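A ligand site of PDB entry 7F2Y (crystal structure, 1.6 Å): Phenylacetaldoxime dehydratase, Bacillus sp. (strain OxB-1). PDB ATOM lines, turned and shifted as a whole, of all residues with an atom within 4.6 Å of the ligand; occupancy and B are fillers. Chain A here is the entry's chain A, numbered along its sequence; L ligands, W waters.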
ATOM      1  N   LEU A 128       3.229 -14.058 -23.162  1.00  0.00           N
ATOM      2  CA  LEU A 128       4.007 -12.982 -22.569  1.00  0.00           C
ATOM      3  C   LEU A 128       5.155 -12.639 -23.519  1.00  0.00           C
ATOM      4  O   LEU A 128       5.714 -13.519 -24.166  1.00  0.00           O
ATOM      5  CB  LEU A 128       4.567 -13.377 -21.207  1.00  0.00           C
ATOM      6  CG  LEU A 128       5.129 -12.221 -20.389  1.00  0.00           C
ATOM      7  CD1 LEU A 128       4.013 -11.244 -19.972  1.00  0.00           C
ATOM      8  CD2 LEU A 128       5.914 -12.733 -19.185  1.00  0.00           C
ATOM      9  N   HIS A 150       3.044  -9.828 -14.470  1.00  0.00           N
ATOM     10  CA  HIS A 150       4.266 -10.571 -14.775  1.00  0.00           C
ATOM     11  C   HIS A 150       5.312 -10.186 -13.743  1.00  0.00           C
ATOM     12  O   HIS A 150       5.113  -9.281 -12.923  1.00  0.00           O
ATOM     13  CB  HIS A 150       4.759 -10.314 -16.203  1.00  0.00           C
ATOM     14  CG  HIS A 150       5.500  -9.031 -16.359  1.00  0.00           C
ATOM     15  ND1 HIS A 150       6.890  -8.961 -16.396  1.00  0.00           N
ATOM     16  CD2 HIS A 150       5.063  -7.749 -16.470  1.00  0.00           C
ATOM     17  CE1 HIS A 150       7.260  -7.700 -16.535  1.00  0.00           C
ATOM     18  NE2 HIS A 150       6.177  -6.954 -16.596  1.00  0.00           N
ATOM     19  N   GLU A 151       6.442 -10.905 -13.784  1.00  0.00           N
ATOM     20  CA  GLU A 151       7.572 -10.698 -12.884  1.00  0.00           C
ATOM     21  C   GLU A 151       7.228 -11.085 -11.442  1.00  0.00           C
ATOM     22  O   GLU A 151       7.670 -10.465 -10.490  1.00  0.00           O
ATOM     23  CB  GLU A 151       8.102  -9.259 -12.950  1.00  0.00           C
ATOM     24  CG  GLU A 151       9.591  -9.146 -12.687  1.00  0.00           C
ATOM     25  CD  GLU A 151      10.103  -7.731 -12.874  1.00  0.00           C
ATOM     26  OE1 GLU A 151      10.156  -6.973 -11.878  1.00  0.00           O
ATOM     27  OE2 GLU A 151      10.451  -7.368 -14.019  1.00  0.00           O
ATOM     28  N   TYR A 152       6.420 -12.145 -11.297  1.00  0.00           N
ATOM     29  CA  TYR A 152       6.235 -12.792 -10.016  1.00  0.00           C
ATOM     30  C   TYR A 152       5.854 -14.239 -10.269  1.00  0.00           C
ATOM     31  O   TYR A 152       5.339 -14.576 -11.329  1.00  0.00           O
ATOM     32  CB  TYR A 152       5.174 -12.094  -9.141  1.00  0.00           C
ATOM     33  CG  TYR A 152       3.755 -12.068  -9.675  1.00  0.00           C
ATOM     34  CD1 TYR A 152       2.884 -13.128  -9.469  1.00  0.00           C
ATOM     35  CD2 TYR A 152       3.271 -10.952 -10.357  1.00  0.00           C
ATOM     36  CE1 TYR A 152       1.583 -13.107  -9.951  1.00  0.00           C
ATOM     37  CE2 TYR A 152       1.976 -10.909 -10.835  1.00  0.00           C
ATOM     38  CZ  TYR A 152       1.129 -11.987 -10.622  1.00  0.00           C
ATOM     39  OH  TYR A 152      -0.176 -11.938 -11.093  1.00  0.00           O
ATOM     40  N   TRP A 153       6.133 -15.093  -9.279  1.00  0.00           N
ATOM     41  CA  TRP A 153       5.792 -16.510  -9.401  1.00  0.00           C
ATOM     42  C   TRP A 153       4.277 -16.664  -9.288  1.00  0.00           C
ATOM     43  O   TRP A 153       3.668 -16.252  -8.292  1.00  0.00           O
ATOM     44  CB  TRP A 153       6.489 -17.335  -8.322  1.00  0.00           C
ATOM     45  CG  TRP A 153       7.982 -17.581  -8.482  1.00  0.00           C
ATOM     46  CD1 TRP A 153       8.831 -18.015  -7.504  1.00  0.00           C
ATOM     47  CD2 TRP A 153       8.796 -17.416  -9.665  1.00  0.00           C
ATOM     48  NE1 TRP A 153      10.103 -18.132  -7.991  1.00  0.00           N
ATOM     49  CE2 TRP A 153      10.108 -17.779  -9.314  1.00  0.00           C
ATOM     50  CE3 TRP A 153       8.537 -17.016 -10.978  1.00  0.00           C
ATOM     51  CZ2 TRP A 153      11.165 -17.736 -10.225  1.00  0.00           C
ATOM     52  CZ3 TRP A 153       9.584 -16.971 -11.891  1.00  0.00           C
ATOM     53  CH2 TRP A 153      10.879 -17.338 -11.507  1.00  0.00           C
ATOM     54  N   GLY A 154       3.683 -17.292 -10.300  1.00  0.00           N
ATOM     55  CA  GLY A 154       2.247 -17.376 -10.389  1.00  0.00           C
ATOM     56  C   GLY A 154       1.639 -16.425 -11.392  1.00  0.00           C
ATOM     57  O   GLY A 154       0.419 -16.457 -11.583  1.00  0.00           O
ATOM     58  N   ALA A 155       2.453 -15.598 -12.049  1.00  0.00           N
ATOM     59  CA  ALA A 155       1.912 -14.645 -13.006  1.00  0.00           C
ATOM     60  C   ALA A 155       1.422 -15.350 -14.261  1.00  0.00           C
ATOM     61  O   ALA A 155       0.402 -14.961 -14.838  1.00  0.00           O
ATOM     62  CB  ALA A 155       2.959 -13.573 -13.343  1.00  0.00           C
ATOM     63  N   MET A 156       2.135 -16.393 -14.689  1.00  0.00           N
ATOM     64  CA  MET A 156       1.649 -17.209 -15.807  1.00  0.00           C
ATOM     65  C   MET A 156       0.257 -17.755 -15.523  1.00  0.00           C
ATOM     66  O   MET A 156      -0.653 -17.625 -16.340  1.00  0.00           O
ATOM     67  CB  MET A 156       2.646 -18.352 -16.086  1.00  0.00           C
ATOM     68  CG  MET A 156       2.057 -19.510 -16.873  1.00  0.00           C
ATOM     69  SD  MET A 156       3.186 -20.911 -17.103  1.00  0.00           S
ATOM     70  CE  MET A 156       3.490 -21.441 -15.430  1.00  0.00           C
ATOM     71  N   ARG A 159      -2.369 -14.985 -15.627  1.00  0.00           N
ATOM     72  CA  ARG A 159      -2.703 -14.495 -16.957  1.00  0.00           C
ATOM     73  C   ARG A 159      -3.647 -15.436 -17.695  1.00  0.00           C
ATOM     74  O   ARG A 159      -4.287 -15.011 -18.667  1.00  0.00           O
ATOM     75  CB  ARG A 159      -1.454 -14.278 -17.802  1.00  0.00           C
ATOM     76  CG  ARG A 159      -0.658 -13.020 -17.413  1.00  0.00           C
ATOM     77  CD  ARG A 159       0.447 -12.687 -18.437  1.00  0.00           C
ATOM     78  NE  ARG A 159       1.346 -13.806 -18.720  1.00  0.00           N
ATOM     79  CZ  ARG A 159       2.417 -14.118 -17.997  1.00  0.00           C
ATOM     80  NH1 ARG A 159       2.714 -13.408 -16.905  1.00  0.00           N
ATOM     81  NH2 ARG A 159       3.182 -15.152 -18.341  1.00  0.00           N
ATOM     82  N   ILE A 200       4.137 -25.492 -23.221  1.00  0.00           N
ATOM     83  CA  ILE A 200       4.823 -24.205 -23.296  1.00  0.00           C
ATOM     84  C   ILE A 200       5.703 -24.164 -24.537  1.00  0.00           C
ATOM     85  O   ILE A 200       6.434 -25.111 -24.829  1.00  0.00           O
ATOM     86  CB  ILE A 200       5.645 -23.890 -22.028  1.00  0.00           C
ATOM     87  CG1 ILE A 200       6.343 -22.524 -22.153  1.00  0.00           C
ATOM     88  CG2 ILE A 200       6.667 -25.017 -21.704  1.00  0.00           C
ATOM     89  CD1 ILE A 200       6.850 -21.952 -20.807  1.00  0.00           C
ATOM     90  N   THR A 202       8.560 -21.539 -25.299  1.00  0.00           N
ATOM     91  CA  THR A 202       9.266 -20.400 -24.733  1.00  0.00           C
ATOM     92  C   THR A 202      10.464 -20.097 -25.613  1.00  0.00           C
ATOM     93  O   THR A 202      11.302 -20.979 -25.858  1.00  0.00           O
ATOM     94  CB  THR A 202       9.674 -20.646 -23.264  1.00  0.00           C
ATOM     95  OG1 THR A 202      10.413 -19.500 -22.806  1.00  0.00           O
ATOM     96  CG2 THR A 202      10.527 -21.911 -23.071  1.00  0.00           C
ATOM     97  N   GLN A 204      13.515 -17.534 -27.652  1.00  0.00           N
ATOM     98  CA  GLN A 204      14.658 -16.641 -27.524  1.00  0.00           C
ATOM     99  C   GLN A 204      14.992 -16.119 -28.910  1.00  0.00           C
ATOM    100  O   GLN A 204      15.120 -16.914 -29.849  1.00  0.00           O
ATOM    101  CB  GLN A 204      15.880 -17.365 -26.951  1.00  0.00           C
ATOM    102  CG  GLN A 204      15.620 -18.135 -25.651  1.00  0.00           C
ATOM    103  CD  GLN A 204      14.857 -19.422 -25.857  1.00  0.00           C
ATOM    104  OE1 GLN A 204      15.071 -20.158 -26.823  1.00  0.00           O
ATOM    105  NE2 GLN A 204      13.939 -19.694 -24.940  1.00  0.00           N
ATOM    106  N   VAL A 221      24.101 -17.385 -21.803  1.00  0.00           N
ATOM    107  CA  VAL A 221      22.730 -17.847 -21.611  1.00  0.00           C
ATOM    108  C   VAL A 221      22.484 -19.180 -22.302  1.00  0.00           C
ATOM    109  O   VAL A 221      22.018 -20.135 -21.673  1.00  0.00           O
ATOM    110  CB  VAL A 221      21.725 -16.801 -22.118  1.00  0.00           C
ATOM    111  CG1 VAL A 221      20.305 -17.271 -21.842  1.00  0.00           C
ATOM    112  CG2 VAL A 221      22.024 -15.458 -21.471  1.00  0.00           C
ATOM    113  N   LEU A 225      20.685 -22.731 -21.116  1.00  0.00           N
ATOM    114  CA  LEU A 225      19.419 -23.160 -21.698  1.00  0.00           C
ATOM    115  C   LEU A 225      19.527 -24.589 -22.215  1.00  0.00           C
ATOM    116  O   LEU A 225      18.609 -25.399 -22.019  1.00  0.00           O
ATOM    117  CB  LEU A 225      19.015 -22.202 -22.819  1.00  0.00           C
ATOM    118  CG  LEU A 225      17.799 -22.612 -23.650  1.00  0.00           C
ATOM    119  CD1 LEU A 225      16.567 -22.729 -22.787  1.00  0.00           C
ATOM    120  CD2 LEU A 225      17.608 -21.592 -24.780  1.00  0.00           C
ATOM    121  N   ALA A 228      19.390 -26.826 -19.360  1.00  0.00           N
ATOM    122  CA  ALA A 228      18.054 -26.937 -18.794  1.00  0.00           C
ATOM    123  C   ALA A 228      17.212 -27.926 -19.593  1.00  0.00           C
ATOM    124  O   ALA A 228      16.562 -28.816 -19.009  1.00  0.00           O
ATOM    125  CB  ALA A 228      17.373 -25.569 -18.758  1.00  0.00           C
ATOM    126  N   LEU A 232      15.506 -31.588 -18.468  1.00  0.00           N
ATOM    127  CA  LEU A 232      14.098 -31.910 -18.596  1.00  0.00           C
ATOM    128  C   LEU A 232      13.891 -33.191 -19.421  1.00  0.00           C
ATOM    129  O   LEU A 232      13.047 -34.022 -19.073  1.00  0.00           O
ATOM    130  CB  LEU A 232      13.360 -30.725 -19.223  1.00  0.00           C
ATOM    131  CG  LEU A 232      13.299 -29.516 -18.282  1.00  0.00           C
ATOM    132  CD1 LEU A 232      13.017 -28.218 -19.060  1.00  0.00           C
ATOM    133  CD2 LEU A 232      12.235 -29.757 -17.203  1.00  0.00           C
ATOM    134  N   VAL A 262      12.192 -23.522 -26.774  1.00  0.00           N
ATOM    135  CA  VAL A 262      11.958 -24.800 -26.109  1.00  0.00           C
ATOM    136  C   VAL A 262      10.458 -25.047 -26.185  1.00  0.00           C
ATOM    137  O   VAL A 262       9.662 -24.156 -25.866  1.00  0.00           O
ATOM    138  CB  VAL A 262      12.458 -24.793 -24.652  1.00  0.00           C
ATOM    139  CG1 VAL A 262      11.982 -26.055 -23.911  1.00  0.00           C
ATOM    140  CG2 VAL A 262      13.968 -24.711 -24.622  1.00  0.00           C
ATOM    141  N   TYR A 266       4.032 -30.719 -19.987  1.00  0.00           N
ATOM    142  CA  TYR A 266       4.139 -31.039 -18.574  1.00  0.00           C
ATOM    143  C   TYR A 266       2.828 -31.671 -18.125  1.00  0.00           C
ATOM    144  O   TYR A 266       1.765 -31.369 -18.673  1.00  0.00           O
ATOM    145  CB  TYR A 266       4.449 -29.764 -17.751  1.00  0.00           C
ATOM    146  CG  TYR A 266       5.831 -29.241 -18.017  1.00  0.00           C
ATOM    147  CD1 TYR A 266       6.110 -28.554 -19.211  1.00  0.00           C
ATOM    148  CD2 TYR A 266       6.856 -29.465 -17.116  1.00  0.00           C
ATOM    149  CE1 TYR A 266       7.380 -28.109 -19.466  1.00  0.00           C
ATOM    150  CE2 TYR A 266       8.136 -29.023 -17.370  1.00  0.00           C
ATOM    151  CZ  TYR A 266       8.398 -28.344 -18.540  1.00  0.00           C
ATOM    152  OH  TYR A 266       9.683 -27.914 -18.789  1.00  0.00           O
ATOM    153  N   LEU A 272       5.261 -27.447 -14.282  1.00  0.00           N
ATOM    154  CA  LEU A 272       6.063 -26.434 -14.965  1.00  0.00           C
ATOM    155  C   LEU A 272       6.460 -25.313 -14.006  1.00  0.00           C
ATOM    156  O   LEU A 272       7.611 -24.873 -14.011  1.00  0.00           O
ATOM    157  CB  LEU A 272       5.274 -25.895 -16.159  1.00  0.00           C
ATOM    158  CG  LEU A 272       5.840 -24.668 -16.870  1.00  0.00           C
ATOM    159  CD1 LEU A 272       7.208 -24.995 -17.435  1.00  0.00           C
ATOM    160  CD2 LEU A 272       4.864 -24.227 -17.965  1.00  0.00           C
ATOM    161  N   TRP A 275       9.266 -26.540 -11.489  1.00  0.00           N
ATOM    162  CA  TRP A 275      10.584 -26.592 -12.125  1.00  0.00           C
ATOM    163  C   TRP A 275      11.134 -25.185 -12.360  1.00  0.00           C
ATOM    164  O   TRP A 275      12.281 -24.889 -12.003  1.00  0.00           O
ATOM    165  CB  TRP A 275      10.532 -27.361 -13.447  1.00  0.00           C
ATOM    166  CG  TRP A 275      11.893 -27.386 -14.091  1.00  0.00           C
ATOM    167  CD1 TRP A 275      12.910 -28.265 -13.836  1.00  0.00           C
ATOM    168  CD2 TRP A 275      12.414 -26.442 -15.054  1.00  0.00           C
ATOM    169  NE1 TRP A 275      14.015 -27.953 -14.596  1.00  0.00           N
ATOM    170  CE2 TRP A 275      13.734 -26.838 -15.351  1.00  0.00           C
ATOM    171  CE3 TRP A 275      11.892 -25.318 -15.688  1.00  0.00           C
ATOM    172  CZ2 TRP A 275      14.541 -26.140 -16.260  1.00  0.00           C
ATOM    173  CZ3 TRP A 275      12.686 -24.629 -16.605  1.00  0.00           C
ATOM    174  CH2 TRP A 275      14.004 -25.048 -16.873  1.00  0.00           C
ATOM    175  N   THR A 276      10.335 -24.319 -12.970  1.00  0.00           N
ATOM    176  CA  THR A 276      10.793 -22.962 -13.256  1.00  0.00           C
ATOM    177  C   THR A 276      11.241 -22.248 -11.986  1.00  0.00           C
ATOM    178  O   THR A 276      12.291 -21.604 -11.965  1.00  0.00           O
ATOM    179  CB  THR A 276       9.682 -22.187 -13.948  1.00  0.00           C
ATOM    180  OG1 THR A 276       9.331 -22.859 -15.153  1.00  0.00           O
ATOM    181  CG2 THR A 276      10.141 -20.774 -14.265  1.00  0.00           C
ATOM    182  N   HIS A 277      10.453 -22.360 -10.916  1.00  0.00           N
ATOM    183  CA  HIS A 277      10.723 -21.626  -9.685  1.00  0.00           C
ATOM    184  C   HIS A 277      11.861 -22.246  -8.867  1.00  0.00           C
ATOM    185  O   HIS A 277      12.468 -21.524  -8.059  1.00  0.00           O
ATOM    186  CB  HIS A 277       9.460 -21.570  -8.813  1.00  0.00           C
ATOM    187  CG  HIS A 277       8.261 -21.012  -9.516  1.00  0.00           C
ATOM    188  ND1 HIS A 277       6.991 -21.114  -9.013  1.00  0.00           N
ATOM    189  CD2 HIS A 277       8.146 -20.350 -10.692  1.00  0.00           C
ATOM    190  CE1 HIS A 277       6.136 -20.550  -9.846  1.00  0.00           C
ATOM    191  NE2 HIS A 277       6.810 -20.068 -10.877  1.00  0.00           N
ATOM    192  N   HIS A 282      17.144 -22.766 -14.485  1.00  0.00           N
ATOM    193  CA  HIS A 282      16.306 -21.605 -14.768  1.00  0.00           C
ATOM    194  C   HIS A 282      16.705 -20.421 -13.886  1.00  0.00           C
ATOM    195  O   HIS A 282      16.656 -19.279 -14.338  1.00  0.00           O
ATOM    196  CB  HIS A 282      14.820 -21.915 -14.618  1.00  0.00           C
ATOM    197  CG  HIS A 282      13.944 -20.845 -15.211  1.00  0.00           C
ATOM    198  ND1 HIS A 282      13.610 -19.698 -14.520  1.00  0.00           N
ATOM    199  CD2 HIS A 282      13.417 -20.710 -16.444  1.00  0.00           C
ATOM    200  CE1 HIS A 282      12.888 -18.918 -15.297  1.00  0.00           C
ATOM    201  NE2 HIS A 282      12.760 -19.508 -16.475  1.00  0.00           N
ATOM    202  N   ILE A 285      19.704 -18.691 -15.794  1.00  0.00           N
ATOM    203  CA  ILE A 285      19.427 -17.925 -17.008  1.00  0.00           C
ATOM    204  C   ILE A 285      18.506 -16.739 -16.719  1.00  0.00           C
ATOM    205  O   ILE A 285      18.630 -15.692 -17.359  1.00  0.00           O
ATOM    206  CB  ILE A 285      18.844 -18.830 -18.099  1.00  0.00           C
ATOM    207  CG1 ILE A 285      17.628 -19.602 -17.593  1.00  0.00           C
ATOM    208  CG2 ILE A 285      19.902 -19.775 -18.617  1.00  0.00           C
ATOM    209  CD1 ILE A 285      17.263 -20.803 -18.457  1.00  0.00           C
ATOM    210  N   TYR A 286      17.567 -16.892 -15.771  1.00  0.00           N
ATOM    211  CA  TYR A 286      16.774 -15.761 -15.337  1.00  0.00           C
ATOM    212  C   TYR A 286      17.669 -14.640 -14.848  1.00  0.00           C
ATOM    213  O   TYR A 286      17.490 -13.470 -15.233  1.00  0.00           O
ATOM    214  CB  TYR A 286      15.813 -16.196 -14.224  1.00  0.00           C
ATOM    215  CG  TYR A 286      14.763 -15.173 -13.797  1.00  0.00           C
ATOM    216  CD1 TYR A 286      15.130 -13.917 -13.327  1.00  0.00           C
ATOM    217  CD2 TYR A 286      13.415 -15.485 -13.830  1.00  0.00           C
ATOM    218  CE1 TYR A 286      14.175 -12.986 -12.936  1.00  0.00           C
ATOM    219  CE2 TYR A 286      12.453 -14.572 -13.433  1.00  0.00           C
ATOM    220  CZ  TYR A 286      12.845 -13.327 -13.000  1.00  0.00           C
ATOM    221  OH  TYR A 286      11.896 -12.408 -12.604  1.00  0.00           O
ATOM    222  N   PHE A 289      19.519 -12.796 -17.754  1.00  0.00           N
ATOM    223  CA  PHE A 289      18.675 -11.885 -18.511  1.00  0.00           C
ATOM    224  C   PHE A 289      18.446 -10.579 -17.765  1.00  0.00           C
ATOM    225  O   PHE A 289      18.445  -9.506 -18.370  1.00  0.00           O
ATOM    226  CB  PHE A 289      17.319 -12.514 -18.823  1.00  0.00           C
ATOM    227  CG  PHE A 289      16.428 -11.617 -19.642  1.00  0.00           C
ATOM    228  CD1 PHE A 289      16.850 -11.183 -20.894  1.00  0.00           C
ATOM    229  CD2 PHE A 289      15.198 -11.204 -19.164  1.00  0.00           C
ATOM    230  CE1 PHE A 289      16.045 -10.360 -21.670  1.00  0.00           C
ATOM    231  CE2 PHE A 289      14.396 -10.369 -19.934  1.00  0.00           C
ATOM    232  CZ  PHE A 289      14.812  -9.956 -21.189  1.00  0.00           C
ATOM    233  N   TYR A 290      18.223 -10.652 -16.451  1.00  0.00           N
ATOM    234  CA  TYR A 290      18.038  -9.409 -15.711  1.00  0.00           C
ATOM    235  C   TYR A 290      19.353  -8.660 -15.552  1.00  0.00           C
ATOM    236  O   TYR A 290      19.322  -7.435 -15.415  1.00  0.00           O
ATOM    237  CB  TYR A 290      17.373  -9.685 -14.361  1.00  0.00           C
ATOM    238  CG  TYR A 290      15.870  -9.569 -14.495  1.00  0.00           C
ATOM    239  CD1 TYR A 290      15.129 -10.588 -15.075  1.00  0.00           C
ATOM    240  CD2 TYR A 290      15.213  -8.407 -14.117  1.00  0.00           C
ATOM    241  CE1 TYR A 290      13.757 -10.473 -15.233  1.00  0.00           C
ATOM    242  CE2 TYR A 290      13.841  -8.293 -14.275  1.00  0.00           C
ATOM    243  CZ  TYR A 290      13.124  -9.323 -14.828  1.00  0.00           C
ATOM    244  OH  TYR A 290      11.765  -9.202 -14.986  1.00  0.00           O
ATOM    245  N   LEU A 304      12.465 -12.136 -25.719  1.00  0.00           N
ATOM    246  CA  LEU A 304      11.963 -13.388 -25.176  1.00  0.00           C
ATOM    247  C   LEU A 304      10.441 -13.370 -25.254  1.00  0.00           C
ATOM    248  O   LEU A 304       9.842 -12.307 -25.199  1.00  0.00           O
ATOM    249  CB  LEU A 304      12.396 -13.619 -23.700  1.00  0.00           C
ATOM    250  CG  LEU A 304      13.877 -13.454 -23.361  1.00  0.00           C
ATOM    251  CD1 LEU A 304      14.051 -13.574 -21.846  1.00  0.00           C
ATOM    252  CD2 LEU A 304      14.655 -14.516 -24.067  1.00  0.00           C
ATOM    253  N   HIS A 306       6.717 -16.215 -24.550  1.00  0.00           N
ATOM    254  CA  HIS A 306       6.223 -17.586 -24.443  1.00  0.00           C
ATOM    255  C   HIS A 306       4.729 -17.631 -24.677  1.00  0.00           C
ATOM    256  O   HIS A 306       4.021 -16.633 -24.605  1.00  0.00           O
ATOM    257  CB  HIS A 306       6.639 -18.251 -23.108  1.00  0.00           C
ATOM    258  CG  HIS A 306       5.795 -17.925 -21.903  1.00  0.00           C
ATOM    259  ND1 HIS A 306       6.316 -17.953 -20.624  1.00  0.00           N
ATOM    260  CD2 HIS A 306       4.458 -17.695 -21.749  1.00  0.00           C
ATOM    261  CE1 HIS A 306       5.369 -17.702 -19.750  1.00  0.00           C
ATOM    262  NE2 HIS A 306       4.227 -17.540 -20.402  1.00  0.00           N
HETATM  263  C1  LIG L   1       9.515 -16.909 -16.513  1.00  0.00           C
HETATM  264  C2  LIG L   1       9.694 -21.425 -18.202  1.00  0.00           C
HETATM  265  C3  LIG L   1      13.869 -20.419 -20.478  1.00  0.00           C
HETATM  266  C4  LIG L   1      13.864 -16.021 -18.480  1.00  0.00           C
HETATM  267  C5  LIG L   1       9.139 -18.181 -16.840  1.00  0.00           C
HETATM  268  C6  LIG L   1       7.864 -18.797 -16.565  1.00  0.00           C
HETATM  269  C7  LIG L   1       7.934 -20.048 -17.032  1.00  0.00           C
HETATM  270  C8  LIG L   1       9.238 -20.261 -17.631  1.00  0.00           C
HETATM  271  C9  LIG L   1       6.831 -21.117 -16.975  1.00  0.00           C
HETATM  272  C10 LIG L   1       6.688 -18.104 -15.834  1.00  0.00           C
HETATM  273  C11 LIG L   1       6.878 -18.242 -14.322  1.00  0.00           C
HETATM  274  C12 LIG L   1       5.627 -17.795 -13.602  1.00  0.00           C
HETATM  275  O1  LIG L   1       5.287 -18.419 -12.553  1.00  0.00           O
HETATM  276  O2  LIG L   1       4.968 -16.841 -14.065  1.00  0.00           O
HETATM  277  C13 LIG L   1      10.851 -21.571 -18.931  1.00  0.00           C
HETATM  278  C14 LIG L   1      11.344 -22.805 -19.538  1.00  0.00           C
HETATM  279  C15 LIG L   1      12.495 -22.512 -20.172  1.00  0.00           C
HETATM  280  C16 LIG L   1      12.783 -21.113 -19.961  1.00  0.00           C
HETATM  281  C17 LIG L   1      10.624 -24.170 -19.468  1.00  0.00           C
HETATM  282  C18 LIG L   1      13.453 -23.427 -20.974  1.00  0.00           C
HETATM  283  C19 LIG L   1      13.660 -24.725 -20.669  1.00  0.00           C
HETATM  284  C20 LIG L   1      14.188 -19.120 -20.198  1.00  0.00           C
HETATM  285  C21 LIG L   1      15.285 -18.363 -20.780  1.00  0.00           C
HETATM  286  C22 LIG L   1      15.282 -17.146 -20.211  1.00  0.00           C
HETATM  287  C23 LIG L   1      14.194 -17.097 -19.261  1.00  0.00           C
HETATM  288  C24 LIG L   1      16.240 -18.930 -21.847  1.00  0.00           C
HETATM  289  C25 LIG L   1      16.208 -15.924 -20.440  1.00  0.00           C
HETATM  290  C26 LIG L   1      17.114 -15.827 -21.423  1.00  0.00           C
HETATM  291  C27 LIG L   1      12.676 -15.871 -17.807  1.00  0.00           C
HETATM  292  C28 LIG L   1      12.180 -14.649 -17.207  1.00  0.00           C
HETATM  293  C29 LIG L   1      10.985 -14.904 -16.675  1.00  0.00           C
HETATM  294  C30 LIG L   1      10.673 -16.293 -16.912  1.00  0.00           C
HETATM  295  C31 LIG L   1      12.938 -13.300 -17.216  1.00  0.00           C
HETATM  296  C32 LIG L   1      10.071 -13.910 -15.921  1.00  0.00           C
HETATM  297  C33 LIG L   1       8.950 -13.477 -16.872  1.00  0.00           C
HETATM  298  C34 LIG L   1       8.025 -12.458 -16.255  1.00  0.00           C
HETATM  299  O3  LIG L   1       7.030 -12.899 -15.622  1.00  0.00           O
HETATM  300  O4  LIG L   1       8.252 -11.235 -16.432  1.00  0.00           O
HETATM  301  N1  LIG L   1       9.955 -19.092 -17.491  1.00  0.00           N
HETATM  302  N2  LIG L   1      11.767 -20.574 -19.207  1.00  0.00           N
HETATM  303  N3  LIG L   1      13.537 -18.315 -19.283  1.00  0.00           N
HETATM  304  N4  LIG L   1      11.733 -16.863 -17.610  1.00  0.00           N
HETATM  305 FE1  LIG L   1      11.797 -18.720 -18.346  1.00  0.00          FE
HETATM  306  O   HOH W   1       5.110 -14.968 -16.040  1.00  0.00           O
HETATM  307  O   HOH W   2       7.550 -14.695 -13.346  1.00  0.00           O
HETATM  308  O   HOH W   3       2.409 -19.245 -12.789  1.00  0.00           O
HETATM  309  O   HOH W   4      10.481  -9.881 -17.302  1.00  0.00           O
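NE2 of Gln 204 is in hydrogen-bond range of O of Thr 202 (3.1 Å). OG1 of Thr 276 sits at hydrogen-bond distance from O of Leu 272. The backbone carbonyl oxygen (O) of Thr 276 sits at hydrogen-bond distance from a ring nitrogen (ND1) of His 282 (3.4 Å). The guanidinium group (NH1) of Arg 159 sits close to the backbone carbonyl oxygen (O) of Ala 155, 3.5 Å away. The side-chain carboxylate of Glu 151 is in hydrogen-bond range of the side-chain hydroxyl of Tyr 290, 2.5 Å away. O of Leu 128 sits at hydrogen-bond distance from N of His 306. The backbone NH of Val 262 lies within hydrogen-bond range of the backbone carbonyl oxygen of Thr 202.
Leu 128 touches the ligand. O of Tyr 152 touches O2 of the ligand, at 3.6 Å. Trp 153 touches the ligand. Ile 200 touches the ligand (CD1 to C2, 3.9 Å). Thr 202 touches the ligand (CG2 to C15, 3.6 Å). NE2 of Gln 204 touches C24 of the ligand (3.9 Å). CG1 of Val 221 touches C26 of the ligand, 3.5 Å away. Leu 225 touches the ligand. CD1 of Leu 232 touches C19 of the ligand, 3.9 Å away. Val 262 touches the ligand. OH of Tyr 266 touches C17 of the ligand (3.9 Å). CG of Leu 272 touches C9 of the ligand, at 3.7 Å. Trp 275 touches the ligand (CZ3 to C17, 3.6 Å). Thr 276 touches the ligand (OG1 to C2, 3.4 Å). Ile 285 touches the ligand (CD1 to C21, 3.9 Å). CE2 of Tyr 286 touches C32 of the ligand, 3.5 Å away. Phe 289 touches the ligand. Tyr 290 touches the ligand. Leu 304 touches the ligand (CD1 to C25, 3.5 Å). 26 residues have an atom within 4 Å of the ligand: Leu 128, His 150, Glu 151, Tyr 152, Trp 153, Gly 154, Ala 155, Met 156, Ile 200, Thr 202, Gln 204, Val 221, Leu 225, Leu 232, Val 262, Tyr 266, Leu 272, Trp 275, Thr 276, His 277, His 282, Ile 285, Tyr 286, Phe 289, Tyr 290 and Leu 304.
Water W1 lies within hydrogen-bond range of an oxygen (O2) of the ligand and the guanidinium group (NH1) of Arg 159. Water W4 lies within hydrogen-bond range of the side-chain hydroxyl of Tyr 290 (2.7 Å) and an oxygen (O4) of the ligand (2.7 Å). Water W2 bridges an oxygen (O3) of the ligand and the backbone carbonyl oxygen (O) of Tyr 152. Water W3 lies within hydrogen-bond range of an oxygen (O1) of the ligand (3.0 Å), the backbone NH (N) of Gly 154 (3.4 Å) and the backbone NH (N) of Met 156 (3.4 Å).
The backbone NH (N) of Ala 155 sits at hydrogen-bond distance from an oxygen (O2) of the ligand (3.5 Å). An oxygen (O2) of the ligand lies within hydrogen-bond range of the backbone NH (N) of Met 156, 2.9 Å away. The backbone NH (N) of Gly 154 lies within hydrogen-bond range of an oxygen (O1) of the ligand, at 3.0 Å. A ring nitrogen (ND1) of His 150 is in hydrogen-bond range of an oxygen (O4) of the ligand (2.7 Å). O1 of the ligand is in hydrogen-bond range of NE2 of His 277 (2.8 Å). An oxygen (O3) of the ligand sits at hydrogen-bond distance from the backbone NH of Glu 151 (2.8 Å). A ring nitrogen (NE2) of His 282 binds an iron atom (FE1) of the ligand.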
